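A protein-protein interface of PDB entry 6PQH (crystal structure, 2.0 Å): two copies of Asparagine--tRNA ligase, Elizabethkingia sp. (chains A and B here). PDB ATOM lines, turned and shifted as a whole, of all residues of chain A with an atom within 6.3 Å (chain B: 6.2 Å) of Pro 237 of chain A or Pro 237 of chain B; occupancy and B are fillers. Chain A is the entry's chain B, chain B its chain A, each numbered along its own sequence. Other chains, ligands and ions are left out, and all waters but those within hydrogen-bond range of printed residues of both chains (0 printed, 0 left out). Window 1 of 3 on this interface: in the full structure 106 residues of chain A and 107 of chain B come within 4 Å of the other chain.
The side-chain carboxylate of Glu 252 of chain A lies within hydrogen-bond range of the backbone NH of Val 170 of chain B (2.8 Å). The backbone NH (N) of Val 170 of chain A is in hydrogen-bond range of the side-chain carboxylate (OE2) of Glu 252 of chain B, 2.9 Å away.
O of Thr 215 of chain B lies within hydrogen-bond range of N of Phe 239 of chain B, at 3.0 Å. O of Val 170 of chain B sits at hydrogen-bond distance from N of Thr 215 of chain B (2.9 Å). N of Phe 239 of chain A sits at hydrogen-bond distance from O of Thr 215 of chain A (3.0 Å). O of Val 170 of chain A lies within hydrogen-bond range of N of Thr 215 of chain A (2.8 Å).
Val 170 of chain A touches Phe 239 of chain B, and with the chains exchanged Phe 239 of chain A touches Val 170 of chain B. Val 170 of chain A touches Glu 252 of chain B, and with the chains exchanged Glu 252 of chain A touches Val 170 of chain B. Phe 235 of chain A touches Trp 254 of chain B, and with the chains exchanged Trp 254 of chain A touches Phe 235 of chain B. Pro 237 of chain A touches Val 170 of chain B, but with the chains exchanged Val 170 of chain A does not touch Pro 237 of chain B (4.02 Å).
Among the printed residues, merely in contact across the chains: Pro 169 of chain A with Glu 252 of chain B (3.3 Å), Val 170 of chain A with Phe 239 of chain B (3.7 Å), Phe 235 of chain A with Trp 254 of chain B (3.7 Å), Pro 237 of chain A with Val 170 of chain B (3.98 Å), Pro 237 of chain A with Pro 237 of chain B (3.6 Å), Phe 239 of chain A with Val 170 of chain B (3.8 Å), Glu 252 of chain A with Pro 169 of chain B (3.2 Å) and Trp 254 of chain A with Phe 235 of chain B (3.6 Å).
Of the printed residues of chain B, Pro 237 of chain A touches Val 170 and Pro 237. Printed residues of chain A within 4 Å of Pro 237 of chain B: Pro 237. Of the printed residues of chain B, Val 170 of chain A touches Phe 239 and Glu 252. Of the printed residues of chain B, Glu 252 of chain A touches Pro 169 and Val 170. Printed residues of chain A within 4 Å of Pro 169 of chain B: Glu 252. Of the printed residues of chain B, Trp 254 of chain A touches Phe 235 (3.6 Å). Printed residues of chain B within 4 Å of Phe 235 of chain A: Trp 254. The nearest residue of chain B that does not touch Pro 237 of chain A is Trp 254 of chain B (4.5 Å).
Hydrophobic or aromatic side chains of chain A that line the printed part of chain B: Pro 169, Val 170, Pro 237, Phe 239 and Trp 254. Of the 12 printed residues of chain B, 7 touch a printed residue of chain A. Among the printed residues, no Asp or Glu carboxylate lies within 4 Å of a Lys or Arg side-chain nitrogen of the other chain.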
ATOM      1  N   PRO A 169      19.683 -15.824   2.585  1.00  0.00           N
ATOM      2  CA  PRO A 169      20.219 -14.512   2.943  1.00  0.00           C
ATOM      3  C   PRO A 169      19.662 -14.010   4.265  1.00  0.00           C
ATOM      4  O   PRO A 169      18.531 -14.310   4.656  1.00  0.00           O
ATOM      5  CB  PRO A 169      19.785 -13.618   1.776  1.00  0.00           C
ATOM      6  CG  PRO A 169      18.566 -14.268   1.260  1.00  0.00           C
ATOM      7  CD  PRO A 169      18.867 -15.744   1.360  1.00  0.00           C
ATOM      8  N   VAL A 170      20.506 -13.263   4.968  1.00  0.00           N
ATOM      9  CA  VAL A 170      20.139 -12.619   6.216  1.00  0.00           C
ATOM     10  C   VAL A 170      19.679 -11.194   5.966  1.00  0.00           C
ATOM     11  O   VAL A 170      18.643 -10.754   6.473  1.00  0.00           O
ATOM     12  CB  VAL A 170      21.340 -12.674   7.191  1.00  0.00           C
ATOM     13  CG1 VAL A 170      21.059 -11.867   8.437  1.00  0.00           C
ATOM     14  CG2 VAL A 170      21.629 -14.084   7.548  1.00  0.00           C
ATOM     15  N   THR A 215      16.273 -10.430   7.983  1.00  0.00           N
ATOM     16  CA  THR A 215      15.224 -11.395   7.678  1.00  0.00           C
ATOM     17  C   THR A 215      14.550 -11.929   8.938  1.00  0.00           C
ATOM     18  O   THR A 215      15.155 -12.034  10.006  1.00  0.00           O
ATOM     19  CB  THR A 215      15.785 -12.571   6.881  1.00  0.00           C
ATOM     20  OG1 THR A 215      14.701 -13.389   6.432  1.00  0.00           O
ATOM     21  CG2 THR A 215      16.728 -13.437   7.747  1.00  0.00           C
ATOM     22  N   SER A 217      12.953 -14.891   8.350  1.00  0.00           N
ATOM     23  CA  SER A 217      12.793 -16.268   7.890  1.00  0.00           C
ATOM     24  C   SER A 217      13.386 -16.437   6.499  1.00  0.00           C
ATOM     25  O   SER A 217      13.157 -15.601   5.619  1.00  0.00           O
ATOM     26  CB  SER A 217      11.312 -16.664   7.849  1.00  0.00           C
ATOM     27  OG  SER A 217      11.173 -17.991   7.369  1.00  0.00           O
ATOM     28  N   PHE A 235      19.522 -23.124   8.511  1.00  0.00           N
ATOM     29  CA  PHE A 235      20.017 -23.242   9.888  1.00  0.00           C
ATOM     30  C   PHE A 235      20.830 -21.966  10.073  1.00  0.00           C
ATOM     31  O   PHE A 235      22.021 -21.923   9.750  1.00  0.00           O
ATOM     32  CB  PHE A 235      20.855 -24.502  10.112  1.00  0.00           C
ATOM     33  CG  PHE A 235      21.148 -24.824  11.574  1.00  0.00           C
ATOM     34  CD1 PHE A 235      20.990 -26.129  12.058  1.00  0.00           C
ATOM     35  CD2 PHE A 235      21.647 -23.859  12.436  1.00  0.00           C
ATOM     36  CE1 PHE A 235      21.283 -26.445  13.381  1.00  0.00           C
ATOM     37  CE2 PHE A 235      21.939 -24.172  13.766  1.00  0.00           C
ATOM     38  CZ  PHE A 235      21.745 -25.467  14.237  1.00  0.00           C
ATOM     39  N   GLY A 236      20.153 -20.914  10.509  1.00  0.00           N
ATOM     40  CA  GLY A 236      20.728 -19.593  10.493  1.00  0.00           C
ATOM     41  C   GLY A 236      19.958 -18.655  11.390  1.00  0.00           C
ATOM     42  O   GLY A 236      18.869 -18.974  11.869  1.00  0.00           O
ATOM     43  N   PRO A 237      20.513 -17.473  11.638  1.00  0.00           N
ATOM     44  CA  PRO A 237      19.858 -16.530  12.541  1.00  0.00           C
ATOM     45  C   PRO A 237      18.720 -15.794  11.853  1.00  0.00           C
ATOM     46  O   PRO A 237      18.740 -15.553  10.643  1.00  0.00           O
ATOM     47  CB  PRO A 237      20.991 -15.569  12.923  1.00  0.00           C
ATOM     48  CG  PRO A 237      21.883 -15.567  11.713  1.00  0.00           C
ATOM     49  CD  PRO A 237      21.815 -16.974  11.159  1.00  0.00           C
ATOM     50  N   THR A 238      17.705 -15.462  12.651  1.00  0.00           N
ATOM     51  CA  THR A 238      16.579 -14.641  12.223  1.00  0.00           C
ATOM     52  C   THR A 238      16.303 -13.606  13.310  1.00  0.00           C
ATOM     53  O   THR A 238      16.800 -13.717  14.434  1.00  0.00           O
ATOM     54  CB  THR A 238      15.331 -15.485  11.940  1.00  0.00           C
ATOM     55  OG1 THR A 238      14.885 -16.085  13.155  1.00  0.00           O
ATOM     56  CG2 THR A 238      15.642 -16.597  10.904  1.00  0.00           C
ATOM     57  N   PHE A 239      15.520 -12.581  12.965  1.00  0.00           N
ATOM     58  CA  PHE A 239      15.451 -11.394  13.804  1.00  0.00           C
ATOM     59  C   PHE A 239      14.037 -10.836  13.847  1.00  0.00           C
ATOM     60  O   PHE A 239      13.348 -10.785  12.825  1.00  0.00           O
ATOM     61  CB  PHE A 239      16.428 -10.320  13.307  1.00  0.00           C
ATOM     62  CG  PHE A 239      17.846 -10.820  13.160  1.00  0.00           C
ATOM     63  CD1 PHE A 239      18.776 -10.620  14.169  1.00  0.00           C
ATOM     64  CD2 PHE A 239      18.236 -11.503  12.020  1.00  0.00           C
ATOM     65  CE1 PHE A 239      20.072 -11.093  14.033  1.00  0.00           C
ATOM     66  CE2 PHE A 239      19.532 -11.995  11.871  1.00  0.00           C
ATOM     67  CZ  PHE A 239      20.451 -11.785  12.878  1.00  0.00           C
ATOM     68  N   GLU A 252      16.953 -11.798  18.473  1.00  0.00           N
ATOM     69  CA  GLU A 252      17.836 -12.505  17.551  1.00  0.00           C
ATOM     70  C   GLU A 252      17.831 -13.969  17.961  1.00  0.00           C
ATOM     71  O   GLU A 252      18.124 -14.284  19.117  1.00  0.00           O
ATOM     72  CB  GLU A 252      19.260 -11.921  17.590  1.00  0.00           C
ATOM     73  CG  GLU A 252      20.376 -12.828  17.038  1.00  0.00           C
ATOM     74  CD  GLU A 252      21.778 -12.223  17.214  1.00  0.00           C
ATOM     75  OE1 GLU A 252      21.957 -11.017  16.957  1.00  0.00           O
ATOM     76  OE2 GLU A 252      22.710 -12.955  17.608  1.00  0.00           O
ATOM     77  N   PHE A 253      17.472 -14.863  17.038  1.00  0.00           N
ATOM     78  CA  PHE A 253      17.398 -16.279  17.383  1.00  0.00           C
ATOM     79  C   PHE A 253      17.644 -17.093  16.125  1.00  0.00           C
ATOM     80  O   PHE A 253      17.690 -16.554  15.016  1.00  0.00           O
ATOM     81  CB  PHE A 253      16.055 -16.632  18.044  1.00  0.00           C
ATOM     82  CG  PHE A 253      14.844 -16.160  17.268  1.00  0.00           C
ATOM     83  CD1 PHE A 253      14.171 -17.024  16.422  1.00  0.00           C
ATOM     84  CD2 PHE A 253      14.396 -14.841  17.378  1.00  0.00           C
ATOM     85  CE1 PHE A 253      13.067 -16.586  15.696  1.00  0.00           C
ATOM     86  CE2 PHE A 253      13.289 -14.397  16.666  1.00  0.00           C
ATOM     87  CZ  PHE A 253      12.620 -15.272  15.822  1.00  0.00           C
ATOM     88  N   TRP A 254      17.804 -18.402  16.306  1.00  0.00           N
ATOM     89  CA  TRP A 254      18.162 -19.301  15.218  1.00  0.00           C
ATOM     90  C   TRP A 254      16.979 -20.176  14.846  1.00  0.00           C
ATOM     91  O   TRP A 254      16.314 -20.742  15.723  1.00  0.00           O
ATOM     92  CB  TRP A 254      19.374 -20.160  15.597  1.00  0.00           C
ATOM     93  CG  TRP A 254      20.620 -19.340  15.655  1.00  0.00           C
ATOM     94  CD1 TRP A 254      20.889 -18.325  16.527  1.00  0.00           C
ATOM     95  CD2 TRP A 254      21.765 -19.454  14.800  1.00  0.00           C
ATOM     96  NE1 TRP A 254      22.133 -17.801  16.273  1.00  0.00           N
ATOM     97  CE2 TRP A 254      22.696 -18.484  15.220  1.00  0.00           C
ATOM     98  CE3 TRP A 254      22.097 -20.294  13.731  1.00  0.00           C
ATOM     99  CZ2 TRP A 254      23.928 -18.310  14.590  1.00  0.00           C
ATOM    100  CZ3 TRP A 254      23.340 -20.127  13.111  1.00  0.00           C
ATOM    101  CH2 TRP A 254      24.233 -19.139  13.542  1.00  0.00           C
ATOM    102  N   MET A 255      16.731 -20.289  13.541  1.00  0.00           N
ATOM    103  CA  MET A 255      15.635 -21.070  12.993  1.00  0.00           C
ATOM    104  C   MET A 255      16.187 -22.148  12.071  1.00  0.00           C
ATOM    105  O   MET A 255      17.073 -21.881  11.246  1.00  0.00           O
ATOM    106  CB  MET A 255      14.683 -20.204  12.191  1.00  0.00           C
ATOM    107  CG  MET A 255      13.946 -19.136  12.983  1.00  0.00           C
ATOM    108  SD  MET A 255      12.657 -19.901  13.960  1.00  0.00           S
ATOM    109  CE  MET A 255      11.597 -20.592  12.688  1.00  0.00           C
ATOM    110  N   PRO B 169      26.884 -13.837  18.888  1.00  0.00           N
ATOM    111  CA  PRO B 169      25.835 -12.895  18.491  1.00  0.00           C
ATOM    112  C   PRO B 169      26.117 -12.253  17.141  1.00  0.00           C
ATOM    113  O   PRO B 169      27.268 -12.025  16.755  1.00  0.00           O
ATOM    114  CB  PRO B 169      25.842 -11.861  19.625  1.00  0.00           C
ATOM    115  CG  PRO B 169      27.219 -11.972  20.221  1.00  0.00           C
ATOM    116  CD  PRO B 169      27.522 -13.427  20.147  1.00  0.00           C
ATOM    117  N   VAL B 170      25.037 -11.996  16.406  1.00  0.00           N
ATOM    118  CA  VAL B 170      25.150 -11.309  15.124  1.00  0.00           C
ATOM    119  C   VAL B 170      24.976  -9.809  15.296  1.00  0.00           C
ATOM    120  O   VAL B 170      25.742  -9.015  14.734  1.00  0.00           O
ATOM    121  CB  VAL B 170      24.139 -11.892  14.113  1.00  0.00           C
ATOM    122  CG1 VAL B 170      24.210 -11.146  12.786  1.00  0.00           C
ATOM    123  CG2 VAL B 170      24.408 -13.385  13.878  1.00  0.00           C
ATOM    124  N   THR B 215      27.804  -7.810  13.115  1.00  0.00           N
ATOM    125  CA  THR B 215      29.157  -8.153  13.521  1.00  0.00           C
ATOM    126  C   THR B 215      30.011  -8.542  12.312  1.00  0.00           C
ATOM    127  O   THR B 215      29.510  -9.019  11.289  1.00  0.00           O
ATOM    128  CB  THR B 215      29.127  -9.284  14.547  1.00  0.00           C
ATOM    129  OG1 THR B 215      30.453  -9.502  15.057  1.00  0.00           O
ATOM    130  CG2 THR B 215      28.622 -10.564  13.903  1.00  0.00           C
ATOM    131  N   PHE B 235      29.885 -20.888  13.375  1.00  0.00           N
ATOM    132  CA  PHE B 235      29.518 -21.238  11.998  1.00  0.00           C
ATOM    133  C   PHE B 235      28.270 -20.385  11.755  1.00  0.00           C
ATOM    134  O   PHE B 235      27.166 -20.775  12.131  1.00  0.00           O
ATOM    135  CB  PHE B 235      29.240 -22.731  11.835  1.00  0.00           C
ATOM    136  CG  PHE B 235      29.147 -23.222  10.396  1.00  0.00           C
ATOM    137  CD1 PHE B 235      29.798 -24.390  10.015  1.00  0.00           C
ATOM    138  CD2 PHE B 235      28.382 -22.561   9.449  1.00  0.00           C
ATOM    139  CE1 PHE B 235      29.715 -24.868   8.709  1.00  0.00           C
ATOM    140  CE2 PHE B 235      28.285 -23.037   8.141  1.00  0.00           C
ATOM    141  CZ  PHE B 235      28.954 -24.193   7.773  1.00  0.00           C
ATOM    142  N   GLY B 236      28.480 -19.194  11.200  1.00  0.00           N
ATOM    143  CA  GLY B 236      27.427 -18.212  11.118  1.00  0.00           C
ATOM    144  C   GLY B 236      27.817 -17.076  10.206  1.00  0.00           C
ATOM    145  O   GLY B 236      28.971 -16.958   9.783  1.00  0.00           O
ATOM    146  N   PRO B 237      26.864 -16.191   9.920  1.00  0.00           N
ATOM    147  CA  PRO B 237      27.125 -15.097   8.984  1.00  0.00           C
ATOM    148  C   PRO B 237      27.857 -13.932   9.626  1.00  0.00           C
ATOM    149  O   PRO B 237      27.721 -13.648  10.816  1.00  0.00           O
ATOM    150  CB  PRO B 237      25.715 -14.682   8.543  1.00  0.00           C
ATOM    151  CG  PRO B 237      24.879 -14.915   9.759  1.00  0.00           C
ATOM    152  CD  PRO B 237      25.456 -16.215  10.354  1.00  0.00           C
ATOM    153  N   THR B 238      28.640 -13.240   8.802  1.00  0.00           N
ATOM    154  CA  THR B 238      29.357 -12.043   9.214  1.00  0.00           C
ATOM    155  C   THR B 238      29.248 -11.044   8.073  1.00  0.00           C
ATOM    156  O   THR B 238      28.916 -11.415   6.947  1.00  0.00           O
ATOM    157  CB  THR B 238      30.823 -12.348   9.561  1.00  0.00           C
ATOM    158  OG1 THR B 238      31.504 -12.810   8.392  1.00  0.00           O
ATOM    159  CG2 THR B 238      30.909 -13.438  10.675  1.00  0.00           C
ATOM    160  N   PHE B 239      29.494  -9.765   8.366  1.00  0.00           N
ATOM    161  CA  PHE B 239      29.114  -8.704   7.435  1.00  0.00           C
ATOM    162  C   PHE B 239      30.172  -7.616   7.361  1.00  0.00           C
ATOM    163  O   PHE B 239      30.718  -7.200   8.389  1.00  0.00           O
ATOM    164  CB  PHE B 239      27.765  -8.088   7.822  1.00  0.00           C
ATOM    165  CG  PHE B 239      26.680  -9.100   8.002  1.00  0.00           C
ATOM    166  CD1 PHE B 239      25.797  -9.386   6.966  1.00  0.00           C
ATOM    167  CD2 PHE B 239      26.564  -9.803   9.192  1.00  0.00           C
ATOM    168  CE1 PHE B 239      24.798 -10.346   7.137  1.00  0.00           C
ATOM    169  CE2 PHE B 239      25.582 -10.783   9.361  1.00  0.00           C
ATOM    170  CZ  PHE B 239      24.691 -11.042   8.330  1.00  0.00           C
ATOM    171  N   GLU B 252      28.029 -10.006   2.764  1.00  0.00           N
ATOM    172  CA  GLU B 252      27.453 -10.955   3.702  1.00  0.00           C
ATOM    173  C   GLU B 252      28.057 -12.292   3.332  1.00  0.00           C
ATOM    174  O   GLU B 252      27.973 -12.703   2.169  1.00  0.00           O
ATOM    175  CB  GLU B 252      25.916 -10.995   3.609  1.00  0.00           C
ATOM    176  CG  GLU B 252      25.264 -12.244   4.229  1.00  0.00           C
ATOM    177  CD  GLU B 252      23.739 -12.263   4.120  1.00  0.00           C
ATOM    178  OE1 GLU B 252      23.089 -11.205   4.333  1.00  0.00           O
ATOM    179  OE2 GLU B 252      23.182 -13.347   3.832  1.00  0.00           O
ATOM    180  N   PHE B 253      28.692 -12.942   4.298  1.00  0.00           N
ATOM    181  CA  PHE B 253      29.360 -14.210   4.048  1.00  0.00           C
ATOM    182  C   PHE B 253      29.450 -14.976   5.359  1.00  0.00           C
ATOM    183  O   PHE B 253      29.208 -14.434   6.440  1.00  0.00           O
ATOM    184  CB  PHE B 253      30.746 -14.006   3.413  1.00  0.00           C
ATOM    185  CG  PHE B 253      31.645 -13.047   4.161  1.00  0.00           C
ATOM    186  CD1 PHE B 253      32.663 -13.519   4.967  1.00  0.00           C
ATOM    187  CD2 PHE B 253      31.491 -11.675   4.027  1.00  0.00           C
ATOM    188  CE1 PHE B 253      33.504 -12.632   5.641  1.00  0.00           C
ATOM    189  CE2 PHE B 253      32.311 -10.797   4.709  1.00  0.00           C
ATOM    190  CZ  PHE B 253      33.322 -11.285   5.515  1.00  0.00           C
ATOM    191  N   TRP B 254      29.797 -16.253   5.255  1.00  0.00           N
ATOM    192  CA  TRP B 254      29.730 -17.160   6.391  1.00  0.00           C
ATOM    193  C   TRP B 254      31.144 -17.463   6.861  1.00  0.00           C
ATOM    194  O   TRP B 254      32.012 -17.772   6.044  1.00  0.00           O
ATOM    195  CB  TRP B 254      28.979 -18.429   5.988  1.00  0.00           C
ATOM    196  CG  TRP B 254      27.518 -18.177   5.950  1.00  0.00           C
ATOM    197  CD1 TRP B 254      26.849 -17.382   5.062  1.00  0.00           C
ATOM    198  CD2 TRP B 254      26.530 -18.693   6.852  1.00  0.00           C
ATOM    199  NE1 TRP B 254      25.509 -17.382   5.348  1.00  0.00           N
ATOM    200  CE2 TRP B 254      25.284 -18.171   6.446  1.00  0.00           C
ATOM    201  CE3 TRP B 254      26.578 -19.548   7.960  1.00  0.00           C
ATOM    202  CZ2 TRP B 254      24.086 -18.471   7.111  1.00  0.00           C
ATOM    203  CZ3 TRP B 254      25.386 -19.857   8.617  1.00  0.00           C
ATOM    204  CH2 TRP B 254      24.157 -19.322   8.187  1.00  0.00           C
ATOM    205  N   MET B 255      31.384 -17.341   8.163  1.00  0.00           N
ATOM    206  CA  MET B 255      32.706 -17.578   8.732  1.00  0.00           C
ATOM    207  C   MET B 255      32.637 -18.720   9.725  1.00  0.00           C
ATOM    208  O   MET B 255      31.692 -18.815  10.515  1.00  0.00           O
ATOM    209  CB  MET B 255      33.269 -16.347   9.455  1.00  0.00           C
ATOM    210  CG  MET B 255      33.620 -15.180   8.535  1.00  0.00           C
ATOM    211  SD  MET B 255      35.054 -15.464   7.476  1.00  0.00           S
ATOM    212  CE  MET B 255      36.369 -15.566   8.692  1.00  0.00           C
